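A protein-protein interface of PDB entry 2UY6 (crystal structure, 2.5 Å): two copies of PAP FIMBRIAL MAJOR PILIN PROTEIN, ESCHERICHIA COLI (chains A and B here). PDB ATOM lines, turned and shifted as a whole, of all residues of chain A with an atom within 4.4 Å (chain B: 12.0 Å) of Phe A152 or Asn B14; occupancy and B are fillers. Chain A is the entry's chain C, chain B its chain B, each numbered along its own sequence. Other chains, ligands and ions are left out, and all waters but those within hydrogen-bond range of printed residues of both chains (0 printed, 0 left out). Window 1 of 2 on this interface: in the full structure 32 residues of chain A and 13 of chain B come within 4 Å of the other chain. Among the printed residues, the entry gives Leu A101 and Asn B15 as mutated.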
ATOM      1  N   ILE A  33       4.582 -24.142   5.411  1.00  0.00           N
ATOM      2  CA  ILE A  33       5.353 -23.768   4.238  1.00  0.00           C
ATOM      3  C   ILE A  33       5.050 -22.300   3.947  1.00  0.00           C
ATOM      4  O   ILE A  33       3.881 -21.894   3.863  1.00  0.00           O
ATOM      5  CB  ILE A  33       4.972 -24.621   3.018  1.00  0.00           C
ATOM      6  CG1 ILE A  33       5.348 -26.080   3.263  1.00  0.00           C
ATOM      7  CG2 ILE A  33       5.701 -24.111   1.777  1.00  0.00           C
ATOM      8  CD1 ILE A  33       4.867 -27.018   2.173  1.00  0.00           C
ATOM      9  N   ASP A  34       6.103 -21.502   3.818  1.00  0.00           N
ATOM     10  CA  ASP A  34       5.946 -20.082   3.546  1.00  0.00           C
ATOM     11  C   ASP A  34       6.566 -19.754   2.195  1.00  0.00           C
ATOM     12  O   ASP A  34       7.783 -19.801   2.032  1.00  0.00           O
ATOM     13  CB  ASP A  34       6.628 -19.247   4.637  1.00  0.00           C
ATOM     14  CG  ASP A  34       6.155 -17.792   4.647  1.00  0.00           C
ATOM     15  OD1 ASP A  34       5.647 -17.304   3.613  1.00  0.00           O
ATOM     16  OD2 ASP A  34       6.299 -17.131   5.696  1.00  0.00           O
ATOM     17  N   PHE A  35       5.721 -19.421   1.226  1.00  0.00           N
ATOM     18  CA  PHE A  35       6.195 -19.082  -0.106  1.00  0.00           C
ATOM     19  C   PHE A  35       6.684 -17.636  -0.179  1.00  0.00           C
ATOM     20  O   PHE A  35       7.282 -17.231  -1.175  1.00  0.00           O
ATOM     21  CB  PHE A  35       5.084 -19.295  -1.131  1.00  0.00           C
ATOM     22  CG  PHE A  35       4.659 -20.726  -1.283  1.00  0.00           C
ATOM     23  CD1 PHE A  35       3.571 -21.223  -0.572  1.00  0.00           C
ATOM     24  CD2 PHE A  35       5.337 -21.575  -2.148  1.00  0.00           C
ATOM     25  CE1 PHE A  35       3.162 -22.547  -0.727  1.00  0.00           C
ATOM     26  CE2 PHE A  35       4.943 -22.896  -2.310  1.00  0.00           C
ATOM     27  CZ  PHE A  35       3.852 -23.383  -1.600  1.00  0.00           C
ATOM     28  N   GLY A  36       6.416 -16.861   0.872  1.00  0.00           N
ATOM     29  CA  GLY A  36       6.849 -15.475   0.903  1.00  0.00           C
ATOM     30  C   GLY A  36       5.928 -14.477   0.217  1.00  0.00           C
ATOM     31  O   GLY A  36       4.726 -14.734   0.061  1.00  0.00           O
ATOM     32  N   THR A  95      -7.529 -21.438  -1.158  1.00  0.00           N
ATOM     33  CA  THR A  95      -6.946 -20.615  -0.117  1.00  0.00           C
ATOM     34  C   THR A  95      -8.004 -19.973   0.754  1.00  0.00           C
ATOM     35  O   THR A  95      -9.018 -19.489   0.262  1.00  0.00           O
ATOM     36  CB  THR A  95      -6.076 -19.506  -0.715  1.00  0.00           C
ATOM     37  OG1 THR A  95      -4.788 -20.039  -1.039  1.00  0.00           O
ATOM     38  CG2 THR A  95      -5.916 -18.361   0.265  1.00  0.00           C
ATOM     39  N   GLY A  97      -9.811 -17.258   2.720  1.00  0.00           N
ATOM     40  CA  GLY A  97      -9.884 -15.827   2.489  1.00  0.00           C
ATOM     41  C   GLY A  97      -9.448 -15.597   1.057  1.00  0.00           C
ATOM     42  O   GLY A  97      -9.074 -16.552   0.374  1.00  0.00           O
ATOM     43  N   GLY A  98      -9.485 -14.352   0.591  1.00  0.00           N
ATOM     44  CA  GLY A  98      -9.082 -14.081  -0.780  1.00  0.00           C
ATOM     45  C   GLY A  98      -9.980 -14.807  -1.767  1.00  0.00           C
ATOM     46  O   GLY A  98     -11.110 -15.162  -1.420  1.00  0.00           O
ATOM     47  N   THR A  99      -9.489 -15.050  -2.981  1.00  0.00           N
ATOM     48  CA  THR A  99     -10.303 -15.725  -3.987  1.00  0.00           C
ATOM     49  C   THR A  99      -9.563 -16.371  -5.159  1.00  0.00           C
ATOM     50  O   THR A  99      -9.858 -17.508  -5.532  1.00  0.00           O
ATOM     51  CB  THR A  99     -11.340 -14.752  -4.597  1.00  0.00           C
ATOM     52  OG1 THR A  99     -10.748 -13.453  -4.737  1.00  0.00           O
ATOM     53  CG2 THR A  99     -12.586 -14.666  -3.732  1.00  0.00           C
ATOM     54  N   LEU A 101      -6.162 -17.273  -5.588  1.00  0.00           N
ATOM     55  CA  LEU A 101      -5.025 -18.170  -5.418  1.00  0.00           C
ATOM     56  C   LEU A 101      -5.371 -19.649  -5.266  1.00  0.00           C
ATOM     57  O   LEU A 101      -6.505 -20.015  -4.964  1.00  0.00           O
ATOM     58  CB  LEU A 101      -4.189 -17.722  -4.220  1.00  0.00           C
ATOM     59  CG  LEU A 101      -3.498 -16.365  -4.346  1.00  0.00           C
ATOM     60  CD1 LEU A 101      -2.631 -16.091  -3.110  1.00  0.00           C
ATOM     61  CD2 LEU A 101      -2.644 -16.371  -5.603  1.00  0.00           C
ATOM     62  N   THR A 148      -5.883 -11.074  -6.020  1.00  0.00           N
ATOM     63  CA  THR A 148      -5.936  -9.826  -5.266  1.00  0.00           C
ATOM     64  C   THR A 148      -4.873  -9.861  -4.169  1.00  0.00           C
ATOM     65  O   THR A 148      -4.462 -10.929  -3.716  1.00  0.00           O
ATOM     66  CB  THR A 148      -7.326  -9.594  -4.651  1.00  0.00           C
ATOM     67  OG1 THR A 148      -7.667 -10.691  -3.796  1.00  0.00           O
ATOM     68  CG2 THR A 148      -8.369  -9.462  -5.751  1.00  0.00           C
ATOM     69  N   GLU A 149      -4.422  -8.692  -3.741  1.00  0.00           N
ATOM     70  CA  GLU A 149      -3.374  -8.650  -2.739  1.00  0.00           C
ATOM     71  C   GLU A 149      -3.811  -8.840  -1.289  1.00  0.00           C
ATOM     72  O   GLU A 149      -4.970  -8.630  -0.938  1.00  0.00           O
ATOM     73  CB  GLU A 149      -2.528  -7.369  -2.910  1.00  0.00           C
ATOM     74  CG  GLU A 149      -3.271  -6.054  -3.147  1.00  0.00           C
ATOM     75  CD  GLU A 149      -3.720  -5.820  -4.599  1.00  0.00           C
ATOM     76  OE1 GLU A 149      -4.844  -6.232  -4.952  1.00  0.00           O
ATOM     77  OE2 GLU A 149      -2.953  -5.217  -5.387  1.00  0.00           O
ATOM     78  N   GLY A 150      -2.861  -9.270  -0.461  1.00  0.00           N
ATOM     79  CA  GLY A 150      -3.126  -9.508   0.947  1.00  0.00           C
ATOM     80  C   GLY A 150      -2.382 -10.735   1.460  1.00  0.00           C
ATOM     81  O   GLY A 150      -1.513 -11.279   0.773  1.00  0.00           O
ATOM     82  N   ALA A 151      -2.707 -11.169   2.675  1.00  0.00           N
ATOM     83  CA  ALA A 151      -2.065 -12.347   3.251  1.00  0.00           C
ATOM     84  C   ALA A 151      -2.993 -13.546   3.063  1.00  0.00           C
ATOM     85  O   ALA A 151      -4.200 -13.456   3.297  1.00  0.00           O
ATOM     86  CB  ALA A 151      -1.778 -12.121   4.716  1.00  0.00           C
ATOM     87  N   PHE A 152      -2.425 -14.662   2.621  1.00  0.00           N
ATOM     88  CA  PHE A 152      -3.206 -15.862   2.376  1.00  0.00           C
ATOM     89  C   PHE A 152      -2.640 -17.079   3.083  1.00  0.00           C
ATOM     90  O   PHE A 152      -1.452 -17.148   3.393  1.00  0.00           O
ATOM     91  CB  PHE A 152      -3.285 -16.154   0.872  1.00  0.00           C
ATOM     92  CG  PHE A 152      -3.857 -15.022   0.061  1.00  0.00           C
ATOM     93  CD1 PHE A 152      -3.054 -13.942  -0.318  1.00  0.00           C
ATOM     94  CD2 PHE A 152      -5.204 -15.007  -0.285  1.00  0.00           C
ATOM     95  CE1 PHE A 152      -3.592 -12.864  -1.025  1.00  0.00           C
ATOM     96  CE2 PHE A 152      -5.753 -13.933  -0.992  1.00  0.00           C
ATOM     97  CZ  PHE A 152      -4.945 -12.859  -1.362  1.00  0.00           C
ATOM     98  N   SER A 153      -3.513 -18.042   3.331  1.00  0.00           N
ATOM     99  CA  SER A 153      -3.129 -19.278   3.986  1.00  0.00           C
ATOM    100  C   SER A 153      -4.084 -20.357   3.513  1.00  0.00           C
ATOM    101  O   SER A 153      -5.268 -20.099   3.284  1.00  0.00           O
ATOM    102  CB  SER A 153      -3.229 -19.147   5.506  1.00  0.00           C
ATOM    103  OG  SER A 153      -4.586 -19.037   5.896  1.00  0.00           O
ATOM    104  N   LYS B  10      -1.261 -32.307   9.423  1.00  0.00           N
ATOM    105  CA  LYS B  10      -1.668 -31.196   8.518  1.00  0.00           C
ATOM    106  C   LYS B  10      -0.498 -30.357   8.014  1.00  0.00           C
ATOM    107  O   LYS B  10       0.580 -30.313   8.623  1.00  0.00           O
ATOM    108  CB  LYS B  10      -2.659 -30.267   9.224  1.00  0.00           C
ATOM    109  CG  LYS B  10      -2.105 -29.573  10.461  1.00  0.00           C
ATOM    110  CD  LYS B  10      -2.976 -28.373  10.822  1.00  0.00           C
ATOM    111  CE  LYS B  10      -2.315 -27.483  11.863  1.00  0.00           C
ATOM    112  NZ  LYS B  10      -3.084 -26.215  12.023  1.00  0.00           N
ATOM    113  N   VAL B  11      -0.723 -29.698   6.884  1.00  0.00           N
ATOM    114  CA  VAL B  11       0.275 -28.823   6.305  1.00  0.00           C
ATOM    115  C   VAL B  11      -0.439 -27.508   6.057  1.00  0.00           C
ATOM    116  O   VAL B  11      -1.552 -27.479   5.536  1.00  0.00           O
ATOM    117  CB  VAL B  11       0.857 -29.398   4.996  1.00  0.00           C
ATOM    118  CG1 VAL B  11      -0.253 -29.814   4.070  1.00  0.00           C
ATOM    119  CG2 VAL B  11       1.749 -28.362   4.315  1.00  0.00           C
ATOM    120  N   THR B  12       0.183 -26.420   6.489  1.00  0.00           N
ATOM    121  CA  THR B  12      -0.395 -25.103   6.306  1.00  0.00           C
ATOM    122  C   THR B  12       0.500 -24.317   5.350  1.00  0.00           C
ATOM    123  O   THR B  12       1.710 -24.199   5.578  1.00  0.00           O
ATOM    124  CB  THR B  12      -0.502 -24.362   7.637  1.00  0.00           C
ATOM    125  OG1 THR B  12      -1.304 -25.129   8.542  1.00  0.00           O
ATOM    126  CG2 THR B  12      -1.150 -22.999   7.435  1.00  0.00           C
ATOM    127  N   PHE B  13      -0.097 -23.809   4.273  1.00  0.00           N
ATOM    128  CA  PHE B  13       0.642 -23.044   3.275  1.00  0.00           C
ATOM    129  C   PHE B  13       0.415 -21.557   3.484  1.00  0.00           C
ATOM    130  O   PHE B  13      -0.720 -21.115   3.655  1.00  0.00           O
ATOM    131  CB  PHE B  13       0.209 -23.437   1.858  1.00  0.00           C
ATOM    132  CG  PHE B  13       0.323 -24.912   1.572  1.00  0.00           C
ATOM    133  CD1 PHE B  13      -0.715 -25.783   1.905  1.00  0.00           C
ATOM    134  CD2 PHE B  13       1.471 -25.433   0.984  1.00  0.00           C
ATOM    135  CE1 PHE B  13      -0.607 -27.151   1.652  1.00  0.00           C
ATOM    136  CE2 PHE B  13       1.588 -26.797   0.727  1.00  0.00           C
ATOM    137  CZ  PHE B  13       0.551 -27.659   1.059  1.00  0.00           C
ATOM    138  N   ASN B  14       1.502 -20.794   3.480  1.00  0.00           N
ATOM    139  CA  ASN B  14       1.411 -19.351   3.667  1.00  0.00           C
ATOM    140  C   ASN B  14       2.087 -18.556   2.562  1.00  0.00           C
ATOM    141  O   ASN B  14       3.138 -18.943   2.042  1.00  0.00           O
ATOM    142  CB  ASN B  14       2.030 -18.944   5.000  1.00  0.00           C
ATOM    143  CG  ASN B  14       1.223 -19.417   6.171  1.00  0.00           C
ATOM    144  OD1 ASN B  14       0.081 -18.998   6.349  1.00  0.00           O
ATOM    145  ND2 ASN B  14       1.804 -20.302   6.982  1.00  0.00           N
ATOM    146  N   ASN B  15       1.480 -17.434   2.207  1.00  0.00           N
ATOM    147  CA  ASN B  15       2.059 -16.586   1.185  1.00  0.00           C
ATOM    148  C   ASN B  15       1.431 -15.213   1.290  1.00  0.00           C
ATOM    149  O   ASN B  15       0.437 -15.022   1.977  1.00  0.00           O
ATOM    150  CB  ASN B  15       1.818 -17.176  -0.207  1.00  0.00           C
ATOM    151  CG  ASN B  15       0.426 -16.894  -0.721  1.00  0.00           C
ATOM    152  OD1 ASN B  15       0.111 -15.764  -1.094  1.00  0.00           O
ATOM    153  ND2 ASN B  15      -0.414 -17.915  -0.746  1.00  0.00           N
ATOM    154  N   THR B  16       2.014 -14.254   0.597  1.00  0.00           N
ATOM    155  CA  THR B  16       1.493 -12.909   0.634  1.00  0.00           C
ATOM    156  C   THR B  16       1.505 -12.353  -0.790  1.00  0.00           C
ATOM    157  O   THR B  16       2.342 -12.741  -1.604  1.00  0.00           O
ATOM    158  CB  THR B  16       2.349 -12.077   1.620  1.00  0.00           C
ATOM    159  OG1 THR B  16       1.494 -11.525   2.629  1.00  0.00           O
ATOM    160  CG2 THR B  16       3.123 -10.990   0.918  1.00  0.00           C
ATOM    161  N   VAL B  17       0.552 -11.486  -1.110  1.00  0.00           N
ATOM    162  CA  VAL B  17       0.500 -10.898  -2.447  1.00  0.00           C
ATOM    163  C   VAL B  17       0.479  -9.370  -2.389  1.00  0.00           C
ATOM    164  O   VAL B  17      -0.311  -8.763  -1.656  1.00  0.00           O
ATOM    165  CB  VAL B  17      -0.740 -11.367  -3.239  1.00  0.00           C
ATOM    166  CG1 VAL B  17      -0.734 -10.730  -4.623  1.00  0.00           C
ATOM    167  CG2 VAL B  17      -0.738 -12.878  -3.374  1.00  0.00           C
ATOM    168  N   VAL B  18       1.355  -8.755  -3.171  1.00  0.00           N
ATOM    169  CA  VAL B  18       1.443  -7.308  -3.206  1.00  0.00           C
ATOM    170  C   VAL B  18       1.457  -6.800  -4.638  1.00  0.00           C
ATOM    171  O   VAL B  18       1.716  -7.553  -5.577  1.00  0.00           O
ATOM    172  CB  VAL B  18       2.733  -6.811  -2.528  1.00  0.00           C
ATOM    173  CG1 VAL B  18       2.759  -7.241  -1.073  1.00  0.00           C
ATOM    174  CG2 VAL B  18       3.951  -7.337  -3.296  1.00  0.00           C
ATOM    175  N   ASP B  19       1.176  -5.512  -4.782  1.00  0.00           N
ATOM    176  CA  ASP B  19       1.183  -4.852  -6.072  1.00  0.00           C
ATOM    177  C   ASP B  19       2.642  -4.442  -6.284  1.00  0.00           C
ATOM    178  O   ASP B  19       3.227  -3.756  -5.446  1.00  0.00           O
ATOM    179  CB  ASP B  19       0.290  -3.621  -6.012  1.00  0.00           C
ATOM    180  CG  ASP B  19       0.016  -3.042  -7.373  1.00  0.00           C
ATOM    181  OD1 ASP B  19      -0.280  -1.832  -7.448  1.00  0.00           O
ATOM    182  OD2 ASP B  19       0.084  -3.796  -8.363  1.00  0.00           O
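Among the printed residues, merely in contact across the chains: Ile A33 with Phe B13, Phe A35 with Phe B13, Gly A36 with Asn B15, Leu A101 with Asn B15, Leu A101 with Val B17, Thr A148 with Val B17, Glu A149 with Val B17, Glu A149 with Val B18, Glu A149 with Asp B19, Gly A150 with Thr B16, Ala A151 with Asn B15, Ala A151 with Thr B16, Phe A152 with Asn B14, Phe A152 with Val B17, Ser A153 with Phe B13 and Ser A153 with Asn B14.
No position is printed for both chains.
OD1 of Asp A34 sits at hydrogen-bond distance from N of Gly A36.
O of Thr B12 lies within hydrogen-bond range of N of Ile A33, at 2.9 Å. The backbone NH (N) of Asn B14 sits at hydrogen-bond distance from the backbone carbonyl oxygen (O) of Ile A33. N of Phe A35 lies within hydrogen-bond range of O of Asn B14 (2.8 Å). O of Asn B15 lies within hydrogen-bond range of N of Phe A152. The backbone carbonyl oxygen of Gly A36 lies within hydrogen-bond range of the backbone NH of Thr B16, at 2.8 Å. The backbone carbonyl oxygen (O) of Gly A150 lies within hydrogen-bond range of the backbone NH (N) of Val B17 (2.8 Å). The side-chain carboxylate (OD1) of Asp A34 sits close to the backbone carbonyl oxygen (O) of Asn B14.
Of chain B, only Asn B14, Asn B15 and Val B17 come within 4 Å of Phe A152. Of the printed residues of chain A, Asn B14 touches Ile A33 (2.6 Å), Asp A34 (3.4 Å), Phe A35 (2.8 Å), Phe A152 (3.6 Å) and Ser A153 (3.4 Å). Of chain B, only Asn B14 comes within 4 Å of Asp A34. Of chain B, only Asn B15 (3.4 Å) and Thr B16 (2.8 Å) come within 4 Å of Gly A36. Gly A97 touches none of the printed residues of chain B. No residue of chain B comes within 4 Å of Gly A98. No residue of chain B comes within 4 Å of Thr A99. Of chain B, only Asn B15 and Val B17 come within 4 Å of Leu A101. Of chain B, only Thr B16 and Val B17 come within 4 Å of Gly A150. Of chain B, only Asn B15 (3.9 Å) and Thr B16 (3.7 Å) come within 4 Å of Ala A151. Of chain B, only Phe B13 (3.0 Å) and Asn B14 (3.4 Å) come within 4 Å of Ser A153. Printed residues of chain A within 4 Å of Thr B12: Ile A33. Of the printed residues of chain A, Thr B16 touches Gly A36, Gly A150 and Ala A151. Lys B10 touches none of the printed residues of chain A. Val B11 touches none of the printed residues of chain A. The nearest residue of chain B that does not touch Phe A152 is Phe B13 (4.04 Å). The nearest residue of chain A that does not touch Asn B14 is Gly A36 (4.1 Å). The nearest printed residue of chain A that does not touch Phe B13 is Phe A152 (4.04 Å).
Of the 10 printed residues of chain B, 8 touch a printed residue of chain A. Of the 15 printed residues of chain A, 11 touch a printed residue of chain B. Printed residues of chain A that touch a printed residue of chain B: Ile A33, Asp A34, Phe A35, Gly A36, Leu A101, Thr A148, Glu A149, Gly A150, Ala A151, Phe A152 and Ser A153. Hydrophobic or aromatic side chains of chain A that line the printed part of chain B: Ile A33, Phe A35, Leu A101, Ala A151 and Phe A152. Among the printed residues, no Asp or Glu carboxylate lies within 4 Å of a Lys or Arg side-chain nitrogen of the other chain.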
